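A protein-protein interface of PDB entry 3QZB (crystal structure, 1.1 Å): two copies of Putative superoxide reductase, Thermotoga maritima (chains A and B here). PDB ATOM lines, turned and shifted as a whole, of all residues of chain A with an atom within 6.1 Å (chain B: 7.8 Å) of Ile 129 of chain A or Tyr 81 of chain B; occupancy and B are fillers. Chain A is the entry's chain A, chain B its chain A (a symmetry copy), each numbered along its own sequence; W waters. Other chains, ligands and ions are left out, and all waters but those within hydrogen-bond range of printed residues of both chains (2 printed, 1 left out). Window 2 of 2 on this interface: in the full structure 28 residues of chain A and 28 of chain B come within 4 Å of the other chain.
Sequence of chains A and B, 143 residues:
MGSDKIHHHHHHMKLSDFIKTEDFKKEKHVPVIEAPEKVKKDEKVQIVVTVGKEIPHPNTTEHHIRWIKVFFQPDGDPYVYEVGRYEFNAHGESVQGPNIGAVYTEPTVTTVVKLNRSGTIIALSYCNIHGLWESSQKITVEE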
ATOM      1  N   GLU A  62      12.411 -14.985   5.373  1.00  0.00           N
ATOM      2  CA  GLU A  62      12.527 -14.059   6.469  1.00  0.00           C
ATOM      3  C   GLU A  62      13.880 -14.037   7.165  1.00  0.00           C
ATOM      4  O   GLU A  62      14.238 -13.013   7.745  1.00  0.00           O
ATOM      5  CB  GLU A  62      11.407 -14.335   7.514  1.00  0.00           C
ATOM      6  CG  GLU A  62       9.989 -14.283   6.947  1.00  0.00           C
ATOM      7  CD  GLU A  62       9.541 -15.515   6.088  1.00  0.00           C
ATOM      8  OE1 GLU A  62      10.169 -16.613   6.100  1.00  0.00           O
ATOM      9  OE2 GLU A  62       8.463 -15.377   5.427  1.00  0.00           O
ATOM     10  N   HIS A  63      14.604 -15.165   7.118  1.00  0.00           N
ATOM     11  CA  HIS A  63      15.822 -15.318   7.922  1.00  0.00           C
ATOM     12  C   HIS A  63      16.806 -16.173   7.142  1.00  0.00           C
ATOM     13  O   HIS A  63      16.589 -17.364   6.946  1.00  0.00           O
ATOM     14  CB  HIS A  63      15.511 -15.973   9.257  1.00  0.00           C
ATOM     15  CG  HIS A  63      16.695 -16.146  10.154  1.00  0.00           C
ATOM     16  ND1 HIS A  63      16.713 -17.103  11.135  1.00  0.00           N
ATOM     17  CD2 HIS A  63      17.917 -15.539  10.179  1.00  0.00           C
ATOM     18  CE1 HIS A  63      17.895 -17.054  11.745  1.00  0.00           C
ATOM     19  NE2 HIS A  63      18.655 -16.104  11.183  1.00  0.00           N
ATOM     20  N   HIS A  64      17.961 -15.596   6.800  1.00  0.00           N
ATOM     21  CA  HIS A  64      18.951 -16.290   5.994  1.00  0.00           C
ATOM     22  C   HIS A  64      20.287 -15.609   6.068  1.00  0.00           C
ATOM     23  O   HIS A  64      20.383 -14.407   6.343  1.00  0.00           O
ATOM     24  CB  HIS A  64      18.468 -16.353   4.518  1.00  0.00           C
ATOM     25  CG  HIS A  64      18.084 -15.002   3.954  1.00  0.00           C
ATOM     26  ND1 HIS A  64      16.768 -14.618   3.830  1.00  0.00           N
ATOM     27  CD2 HIS A  64      18.814 -13.957   3.510  1.00  0.00           C
ATOM     28  CE1 HIS A  64      16.739 -13.391   3.332  1.00  0.00           C
ATOM     29  NE2 HIS A  64      17.959 -12.950   3.166  1.00  0.00           N
ATOM     30  N   TYR A 126      27.403 -12.443   7.088  1.00  0.00           N
ATOM     31  CA  TYR A 126      26.306 -11.552   7.427  1.00  0.00           C
ATOM     32  C   TYR A 126      24.988 -12.308   7.327  1.00  0.00           C
ATOM     33  O   TYR A 126      24.654 -12.855   6.290  1.00  0.00           O
ATOM     34  CB  TYR A 126      26.294 -10.349   6.450  1.00  0.00           C
ATOM     35  CG  TYR A 126      25.184  -9.371   6.730  1.00  0.00           C
ATOM     36  CD1 TYR A 126      25.114  -8.672   7.924  1.00  0.00           C
ATOM     37  CD2 TYR A 126      24.190  -9.188   5.823  1.00  0.00           C
ATOM     38  CE1 TYR A 126      24.037  -7.834   8.190  1.00  0.00           C
ATOM     39  CE2 TYR A 126      23.099  -8.341   6.068  1.00  0.00           C
ATOM     40  CZ  TYR A 126      23.041  -7.691   7.262  1.00  0.00           C
ATOM     41  OH  TYR A 126      21.952  -6.878   7.583  1.00  0.00           O
ATOM     42  N   CYS A 127      24.237 -12.268   8.442  1.00  0.00           N
ATOM     43  CA  CYS A 127      22.857 -12.750   8.526  1.00  0.00           C
ATOM     44  C   CYS A 127      21.941 -11.565   8.390  1.00  0.00           C
ATOM     45  O   CYS A 127      22.235 -10.468   8.853  1.00  0.00           O
ATOM     46  CB  CYS A 127      22.679 -13.444   9.875  1.00  0.00           C
ATOM     47  SG  CYS A 127      20.930 -13.941  10.105  1.00  0.00           S
ATOM     48  N   ASN A 128      20.833 -11.764   7.701  1.00  0.00           N
ATOM     49  CA  ASN A 128      19.886 -10.648   7.480  1.00  0.00           C
ATOM     50  C   ASN A 128      19.252 -10.107   8.769  1.00  0.00           C
ATOM     51  O   ASN A 128      18.784  -8.967   8.758  1.00  0.00           O
ATOM     52  CB  ASN A 128      18.829 -10.967   6.440  1.00  0.00           C
ATOM     53  CG  ASN A 128      17.760 -11.903   6.930  1.00  0.00           C
ATOM     54  OD1 ASN A 128      18.005 -12.773   7.771  1.00  0.00           O
ATOM     55  ND2 ASN A 128      16.549 -11.767   6.374  1.00  0.00           N
ATOM     56  N   ILE A 129      19.285 -10.872   9.880  1.00  0.00           N
ATOM     57  CA  ILE A 129      18.748 -10.376  11.136  1.00  0.00           C
ATOM     58  C   ILE A 129      19.704 -10.493  12.310  1.00  0.00           C
ATOM     59  O   ILE A 129      19.448  -9.915  13.352  1.00  0.00           O
ATOM     60  CB  ILE A 129      17.372 -11.050  11.482  1.00  0.00           C
ATOM     61  CG1 ILE A 129      17.541 -12.518  11.834  1.00  0.00           C
ATOM     62  CG2 ILE A 129      16.390 -10.797  10.362  1.00  0.00           C
ATOM     63  CD1 ILE A 129      16.220 -13.248  12.122  1.00  0.00           C
ATOM     64  N   HIS A 130      20.832 -11.232  12.187  1.00  0.00           N
ATOM     65  CA  HIS A 130      21.760 -11.421  13.279  1.00  0.00           C
ATOM     66  C   HIS A 130      23.159 -10.831  13.016  1.00  0.00           C
ATOM     67  O   HIS A 130      24.137 -11.193  13.692  1.00  0.00           O
ATOM     68  CB  HIS A 130      21.913 -12.903  13.635  1.00  0.00           C
ATOM     69  CG  HIS A 130      20.633 -13.528  14.119  1.00  0.00           C
ATOM     70  ND1 HIS A 130      20.019 -14.604  13.479  1.00  0.00           N
ATOM     71  CD2 HIS A 130      19.871 -13.244  15.218  1.00  0.00           C
ATOM     72  CE1 HIS A 130      18.946 -14.924  14.172  1.00  0.00           C
ATOM     73  NE2 HIS A 130      18.823 -14.138  15.218  1.00  0.00           N
ATOM     74  N   GLY A 131      23.230  -9.896  12.068  1.00  0.00           N
ATOM     75  CA  GLY A 131      24.446  -9.122  11.885  1.00  0.00           C
ATOM     76  C   GLY A 131      25.671  -9.906  11.446  1.00  0.00           C
ATOM     77  O   GLY A 131      25.582 -10.888  10.702  1.00  0.00           O
ATOM     78  N   VAL B  70      27.338   0.606   3.560  1.00  0.00           N
ATOM     79  CA  VAL B  70      26.739   1.353   4.646  1.00  0.00           C
ATOM     80  C   VAL B  70      25.992   0.358   5.532  1.00  0.00           C
ATOM     81  O   VAL B  70      25.309  -0.523   5.045  1.00  0.00           O
ATOM     82  CB  VAL B  70      25.805   2.413   4.127  1.00  0.00           C
ATOM     83  CG1 VAL B  70      25.019   3.135   5.270  1.00  0.00           C
ATOM     84  CG2 VAL B  70      26.568   3.453   3.259  1.00  0.00           C
ATOM     85  N   PHE B  71      26.178   0.508   6.833  1.00  0.00           N
ATOM     86  CA  PHE B  71      25.445  -0.224   7.845  1.00  0.00           C
ATOM     87  C   PHE B  71      24.603   0.770   8.669  1.00  0.00           C
ATOM     88  O   PHE B  71      24.992   1.922   8.862  1.00  0.00           O
ATOM     89  CB  PHE B  71      26.383  -0.982   8.788  1.00  0.00           C
ATOM     90  CG  PHE B  71      27.100  -2.137   8.095  1.00  0.00           C
ATOM     91  CD1 PHE B  71      26.528  -3.402   8.055  1.00  0.00           C
ATOM     92  CD2 PHE B  71      28.359  -1.948   7.534  1.00  0.00           C
ATOM     93  CE1 PHE B  71      27.148  -4.431   7.424  1.00  0.00           C
ATOM     94  CE2 PHE B  71      29.031  -3.012   6.899  1.00  0.00           C
ATOM     95  CZ  PHE B  71      28.425  -4.248   6.872  1.00  0.00           C
ATOM     96  N   PHE B  72      23.516   0.240   9.207  1.00  0.00           N
ATOM     97  CA  PHE B  72      22.710   0.959  10.181  1.00  0.00           C
ATOM     98  C   PHE B  72      22.680   0.141  11.471  1.00  0.00           C
ATOM     99  O   PHE B  72      22.367  -1.050  11.447  1.00  0.00           O
ATOM    100  CB  PHE B  72      21.302   1.194   9.675  1.00  0.00           C
ATOM    101  CG  PHE B  72      20.458   2.020  10.590  1.00  0.00           C
ATOM    102  CD1 PHE B  72      20.746   3.353  10.819  1.00  0.00           C
ATOM    103  CD2 PHE B  72      19.383   1.485  11.289  1.00  0.00           C
ATOM    104  CE1 PHE B  72      19.984   4.136  11.677  1.00  0.00           C
ATOM    105  CE2 PHE B  72      18.646   2.262  12.138  1.00  0.00           C
ATOM    106  CZ  PHE B  72      18.929   3.584  12.320  1.00  0.00           C
ATOM    107  N   GLN B  73      22.975   0.814  12.583  1.00  0.00           N
ATOM    108  CA  GLN B  73      22.991   0.210  13.917  1.00  0.00           C
ATOM    109  C   GLN B  73      21.847   0.841  14.721  1.00  0.00           C
ATOM    110  O   GLN B  73      21.999   1.996  15.143  1.00  0.00           O
ATOM    111  CB  GLN B  73      24.338   0.439  14.594  1.00  0.00           C
ATOM    112  CG  GLN B  73      24.685  -0.582  15.656  1.00  0.00           C
ATOM    113  CD  GLN B  73      23.759  -0.514  16.828  1.00  0.00           C
ATOM    114  OE1 GLN B  73      23.724   0.510  17.522  1.00  0.00           O
ATOM    115  NE2 GLN B  73      23.023  -1.571  17.079  1.00  0.00           N
ATOM    116  N   PRO B  74      20.730   0.142  14.940  1.00  0.00           N
ATOM    117  CA  PRO B  74      19.633   0.775  15.676  1.00  0.00           C
ATOM    118  C   PRO B  74      19.971   0.857  17.162  1.00  0.00           C
ATOM    119  O   PRO B  74      20.413  -0.146  17.745  1.00  0.00           O
ATOM    120  CB  PRO B  74      18.445  -0.145  15.422  1.00  0.00           C
ATOM    121  CG  PRO B  74      18.846  -1.044  14.276  1.00  0.00           C
ATOM    122  CD  PRO B  74      20.332  -1.164  14.404  1.00  0.00           C
ATOM    123  N   ASP B  77      19.733  -2.145  19.848  1.00  0.00           N
ATOM    124  CA  ASP B  77      19.684  -3.450  19.169  1.00  0.00           C
ATOM    125  C   ASP B  77      21.062  -4.099  19.199  1.00  0.00           C
ATOM    126  O   ASP B  77      22.082  -3.391  19.170  1.00  0.00           O
ATOM    127  CB  ASP B  77      19.222  -3.236  17.746  1.00  0.00           C
ATOM    128  CG  ASP B  77      18.890  -4.501  17.015  1.00  0.00           C
ATOM    129  OD1 ASP B  77      17.805  -5.074  17.273  1.00  0.00           O
ATOM    130  OD2 ASP B  77      19.760  -4.958  16.212  1.00  0.00           O
ATOM    131  N   PRO B  78      21.150  -5.445  19.177  1.00  0.00           N
ATOM    132  CA  PRO B  78      22.480  -6.067  19.231  1.00  0.00           C
ATOM    133  C   PRO B  78      23.309  -5.985  17.933  1.00  0.00           C
ATOM    134  O   PRO B  78      24.488  -6.364  17.973  1.00  0.00           O
ATOM    135  CB  PRO B  78      22.153  -7.545  19.522  1.00  0.00           C
ATOM    136  CG  PRO B  78      20.794  -7.571  20.091  1.00  0.00           C
ATOM    137  CD  PRO B  78      20.091  -6.451  19.411  1.00  0.00           C
ATOM    138  N   TYR B  79      22.698  -5.638  16.819  1.00  0.00           N
ATOM    139  CA  TYR B  79      23.257  -5.939  15.509  1.00  0.00           C
ATOM    140  C   TYR B  79      23.456  -4.671  14.656  1.00  0.00           C
ATOM    141  O   TYR B  79      22.875  -3.623  14.920  1.00  0.00           O
ATOM    142  CB  TYR B  79      22.364  -6.947  14.781  1.00  0.00           C
ATOM    143  CG  TYR B  79      22.089  -8.197  15.598  1.00  0.00           C
ATOM    144  CD1 TYR B  79      23.122  -9.060  15.969  1.00  0.00           C
ATOM    145  CD2 TYR B  79      20.832  -8.493  16.029  1.00  0.00           C
ATOM    146  CE1 TYR B  79      22.878 -10.182  16.718  1.00  0.00           C
ATOM    147  CE2 TYR B  79      20.563  -9.601  16.813  1.00  0.00           C
ATOM    148  CZ  TYR B  79      21.605 -10.434  17.179  1.00  0.00           C
ATOM    149  OH  TYR B  79      21.366 -11.562  17.943  1.00  0.00           O
ATOM    150  N   VAL B  80      24.207  -4.852  13.542  1.00  0.00           N
ATOM    151  CA  VAL B  80      24.139  -3.984  12.419  1.00  0.00           C
ATOM    152  C   VAL B  80      23.377  -4.616  11.279  1.00  0.00           C
ATOM    153  O   VAL B  80      23.298  -5.858  11.161  1.00  0.00           O
ATOM    154  CB  VAL B  80      25.522  -3.543  11.894  1.00  0.00           C
ATOM    155  CG1 VAL B  80      26.196  -2.606  12.890  1.00  0.00           C
ATOM    156  CG2 VAL B  80      26.459  -4.726  11.581  1.00  0.00           C
ATOM    157  N   TYR B  81      22.861  -3.750  10.376  1.00  0.00           N
ATOM    158  CA  TYR B  81      22.139  -4.124   9.210  1.00  0.00           C
ATOM    159  C   TYR B  81      22.801  -3.484   8.019  1.00  0.00           C
ATOM    160  O   TYR B  81      23.072  -2.283   8.029  1.00  0.00           O
ATOM    161  CB  TYR B  81      20.637  -3.743   9.295  1.00  0.00           C
ATOM    162  CG  TYR B  81      20.017  -4.332  10.540  1.00  0.00           C
ATOM    163  CD1 TYR B  81      19.508  -5.594  10.551  1.00  0.00           C
ATOM    164  CD2 TYR B  81      20.150  -3.691  11.746  1.00  0.00           C
ATOM    165  CE1 TYR B  81      19.047  -6.173  11.743  1.00  0.00           C
ATOM    166  CE2 TYR B  81      19.690  -4.256  12.896  1.00  0.00           C
ATOM    167  CZ  TYR B  81      19.121  -5.498  12.893  1.00  0.00           C
ATOM    168  OH  TYR B  81      18.680  -6.092  14.070  1.00  0.00           O
ATOM    169  N   GLU B  82      23.088  -4.284   6.991  1.00  0.00           N
ATOM    170  CA  GLU B  82      23.724  -3.768   5.785  1.00  0.00           C
ATOM    171  C   GLU B  82      22.671  -3.010   4.981  1.00  0.00           C
ATOM    172  O   GLU B  82      21.741  -3.587   4.429  1.00  0.00           O
ATOM    173  CB  GLU B  82      24.319  -4.908   4.946  1.00  0.00           C
ATOM    174  CG  GLU B  82      25.228  -4.385   3.811  1.00  0.00           C
ATOM    175  CD  GLU B  82      25.877  -5.492   3.024  1.00  0.00           C
ATOM    176  OE1 GLU B  82      25.116  -6.313   2.445  1.00  0.00           O
ATOM    177  OE2 GLU B  82      27.140  -5.523   2.960  1.00  0.00           O
ATOM    178  N   VAL B  83      22.797  -1.706   4.958  1.00  0.00           N
ATOM    179  CA  VAL B  83      21.951  -0.852   4.126  1.00  0.00           C
ATOM    180  C   VAL B  83      22.191  -1.120   2.637  1.00  0.00           C
ATOM    181  O   VAL B  83      21.277  -1.215   1.851  1.00  0.00           O
ATOM    182  CB  VAL B  83      22.189   0.631   4.478  1.00  0.00           C
ATOM    183  CG1 VAL B  83      21.622   1.600   3.449  1.00  0.00           C
ATOM    184  CG2 VAL B  83      21.646   0.923   5.880  1.00  0.00           C
ATOM    185  N   GLY B  84      23.476  -1.288   2.266  1.00  0.00           N
ATOM    186  CA  GLY B  84      23.810  -1.543   0.890  1.00  0.00           C
ATOM    187  C   GLY B  84      25.315  -1.659   0.714  1.00  0.00           C
ATOM    188  O   GLY B  84      26.052  -1.285   1.575  1.00  0.00           O
ATOM    189  N   ARG B 117      13.518   3.897  13.552  1.00  0.00           N
ATOM    190  CA  ARG B 117      14.078   4.090  14.857  1.00  0.00           C
ATOM    191  C   ARG B 117      15.436   4.773  14.739  1.00  0.00           C
ATOM    192  O   ARG B 117      16.144   4.561  13.768  1.00  0.00           O
ATOM    193  CB  ARG B 117      14.274   2.738  15.633  1.00  0.00           C
ATOM    194  CG  ARG B 117      13.076   1.762  15.643  1.00  0.00           C
ATOM    195  CD  ARG B 117      13.081   0.762  16.782  1.00  0.00           C
ATOM    196  NE  ARG B 117      14.231  -0.140  16.818  1.00  0.00           N
ATOM    197  CZ  ARG B 117      14.262  -1.382  16.335  1.00  0.00           C
ATOM    198  NH1 ARG B 117      13.327  -1.878  15.525  1.00  0.00           N
ATOM    199  NH2 ARG B 117      15.268  -2.123  16.678  1.00  0.00           N
ATOM    200  N   THR B 120      22.774   4.637  14.355  1.00  0.00           N
ATOM    201  CA  THR B 120      24.057   5.099  13.863  1.00  0.00           C
ATOM    202  C   THR B 120      24.278   4.587  12.471  1.00  0.00           C
ATOM    203  O   THR B 120      24.088   3.408  12.194  1.00  0.00           O
ATOM    204  CB  THR B 120      25.187   4.667  14.772  1.00  0.00           C
ATOM    205  OG1 THR B 120      24.926   5.113  16.106  1.00  0.00           O
ATOM    206  CG2 THR B 120      26.529   5.229  14.355  1.00  0.00           C
ATOM    207  N   ILE B 122      27.048   3.762   9.716  1.00  0.00           N
ATOM    208  CA  ILE B 122      28.454   3.379   9.619  1.00  0.00           C
ATOM    209  C   ILE B 122      28.798   3.191   8.142  1.00  0.00           C
ATOM    210  O   ILE B 122      28.121   2.461   7.428  1.00  0.00           O
ATOM    211  CB  ILE B 122      28.768   2.112  10.420  1.00  0.00           C
ATOM    212  CG1 ILE B 122      28.377   2.228  11.914  1.00  0.00           C
ATOM    213  CG2 ILE B 122      30.262   1.793  10.310  1.00  0.00           C
ATOM    214  CD1 ILE B 122      28.463   0.895  12.654  1.00  0.00           C
HETATM  215  O   HOH W   1      20.565  -6.109   5.671  1.00  0.00           O
HETATM  216  O   HOH W   2      17.326  -8.401  14.275  1.00  0.00           O
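The side-chain amide nitrogen (ND2) of Asn 128 of chain A lies within hydrogen-bond range of the backbone carbonyl oxygen (O) of Glu 62 of chain A, 3.0 Å away.
OD1 of Asn 128 of chain A lies within hydrogen-bond range of N of His 64 of chain A (3.0 Å).
SG of Cys 127 of chain A lies close to N of Ile 129 of chain A (3.5 Å).
The side-chain amide nitrogen (NE2) of Gln 73 of chain B sits at hydrogen-bond distance from the backbone carbonyl oxygen (O) of Tyr 79 of chain B (3.0 Å).
The backbone NH (N) of Tyr 79 of chain B is in hydrogen-bond range of the side-chain carboxylate (OD2) of Asp 77 of chain B (3.1 Å).
The side-chain carboxylate of Asp 77 of chain B sits at hydrogen-bond distance from the side-chain hydroxyl of Tyr 81 of chain B (2.7 Å).
Water W1 bridges OH of Tyr 126 of chain A (2.5 Å) and O of Glu 82 of chain B (3.0 Å).
Water W2 bridges OH of Tyr 81 of chain B (2.7 Å) and O of Ile 129 of chain A (2.8 Å).
Ile 129 of chain A touches just these residues of chain B: Tyr 79 and Tyr 81.
Of the printed residues of chain B, His 130 of chain A touches Tyr 79.
Of the printed residues of chain A, Tyr 79 of chain B touches Ile 129 (3.3 Å), His 130 (3.3 Å) and Gly 131 (3.99 Å).
Tyr 81 of chain B touches just these residues of chain A: Tyr 126, Asn 128 and Ile 129.
Of the printed residues of chain A, Glu 82 of chain B touches Tyr 126.
Gly 84 of chain B touches none of the printed residues of chain A.
The nearest residue of chain B that does not touch Ile 129 of chain A is Asp 77 of chain B (5.7 Å).
The nearest residue of chain A that does not touch Tyr 81 of chain B is His 130 of chain A (5.4 Å).
The nearest printed residue of chain A that does not touch Glu 82 of chain B is Cys 127 of chain A (6.5 Å).
Of the 9 printed residues of chain A, 5 touch a printed residue of chain B.
Hydrophobic or aromatic side chains of chain A within 4 Å of the printed part of chain B: Tyr 126 and His 130.
Hydrophobic or aromatic side chains of chain B that line the printed part of chain A: Tyr 79 and Tyr 81.
Along chain B the printed residues that touch a printed residue of chain A span positions 79 to 82.
No position is printed for both chains.
Among the printed residues, merely in contact across the chains: Tyr 126 of chain A with Val 80 of chain B, Tyr 126 of chain A with Tyr 81 of chain B, Asn 128 of chain A with Tyr 81 of chain B, Ile 129 of chain A with Tyr 79 of chain B, Ile 129 of chain A with Tyr 81 of chain B, His 130 of chain A with Tyr 79 of chain B, Gly 131 of chain A with Tyr 79 of chain B and Gly 131 of chain A with Val 80 of chain B.
The backbone NH (N) of Glu 82 of chain B is in hydrogen-bond range of the side-chain hydroxyl (OH) of Tyr 126 of chain A (2.9 Å).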
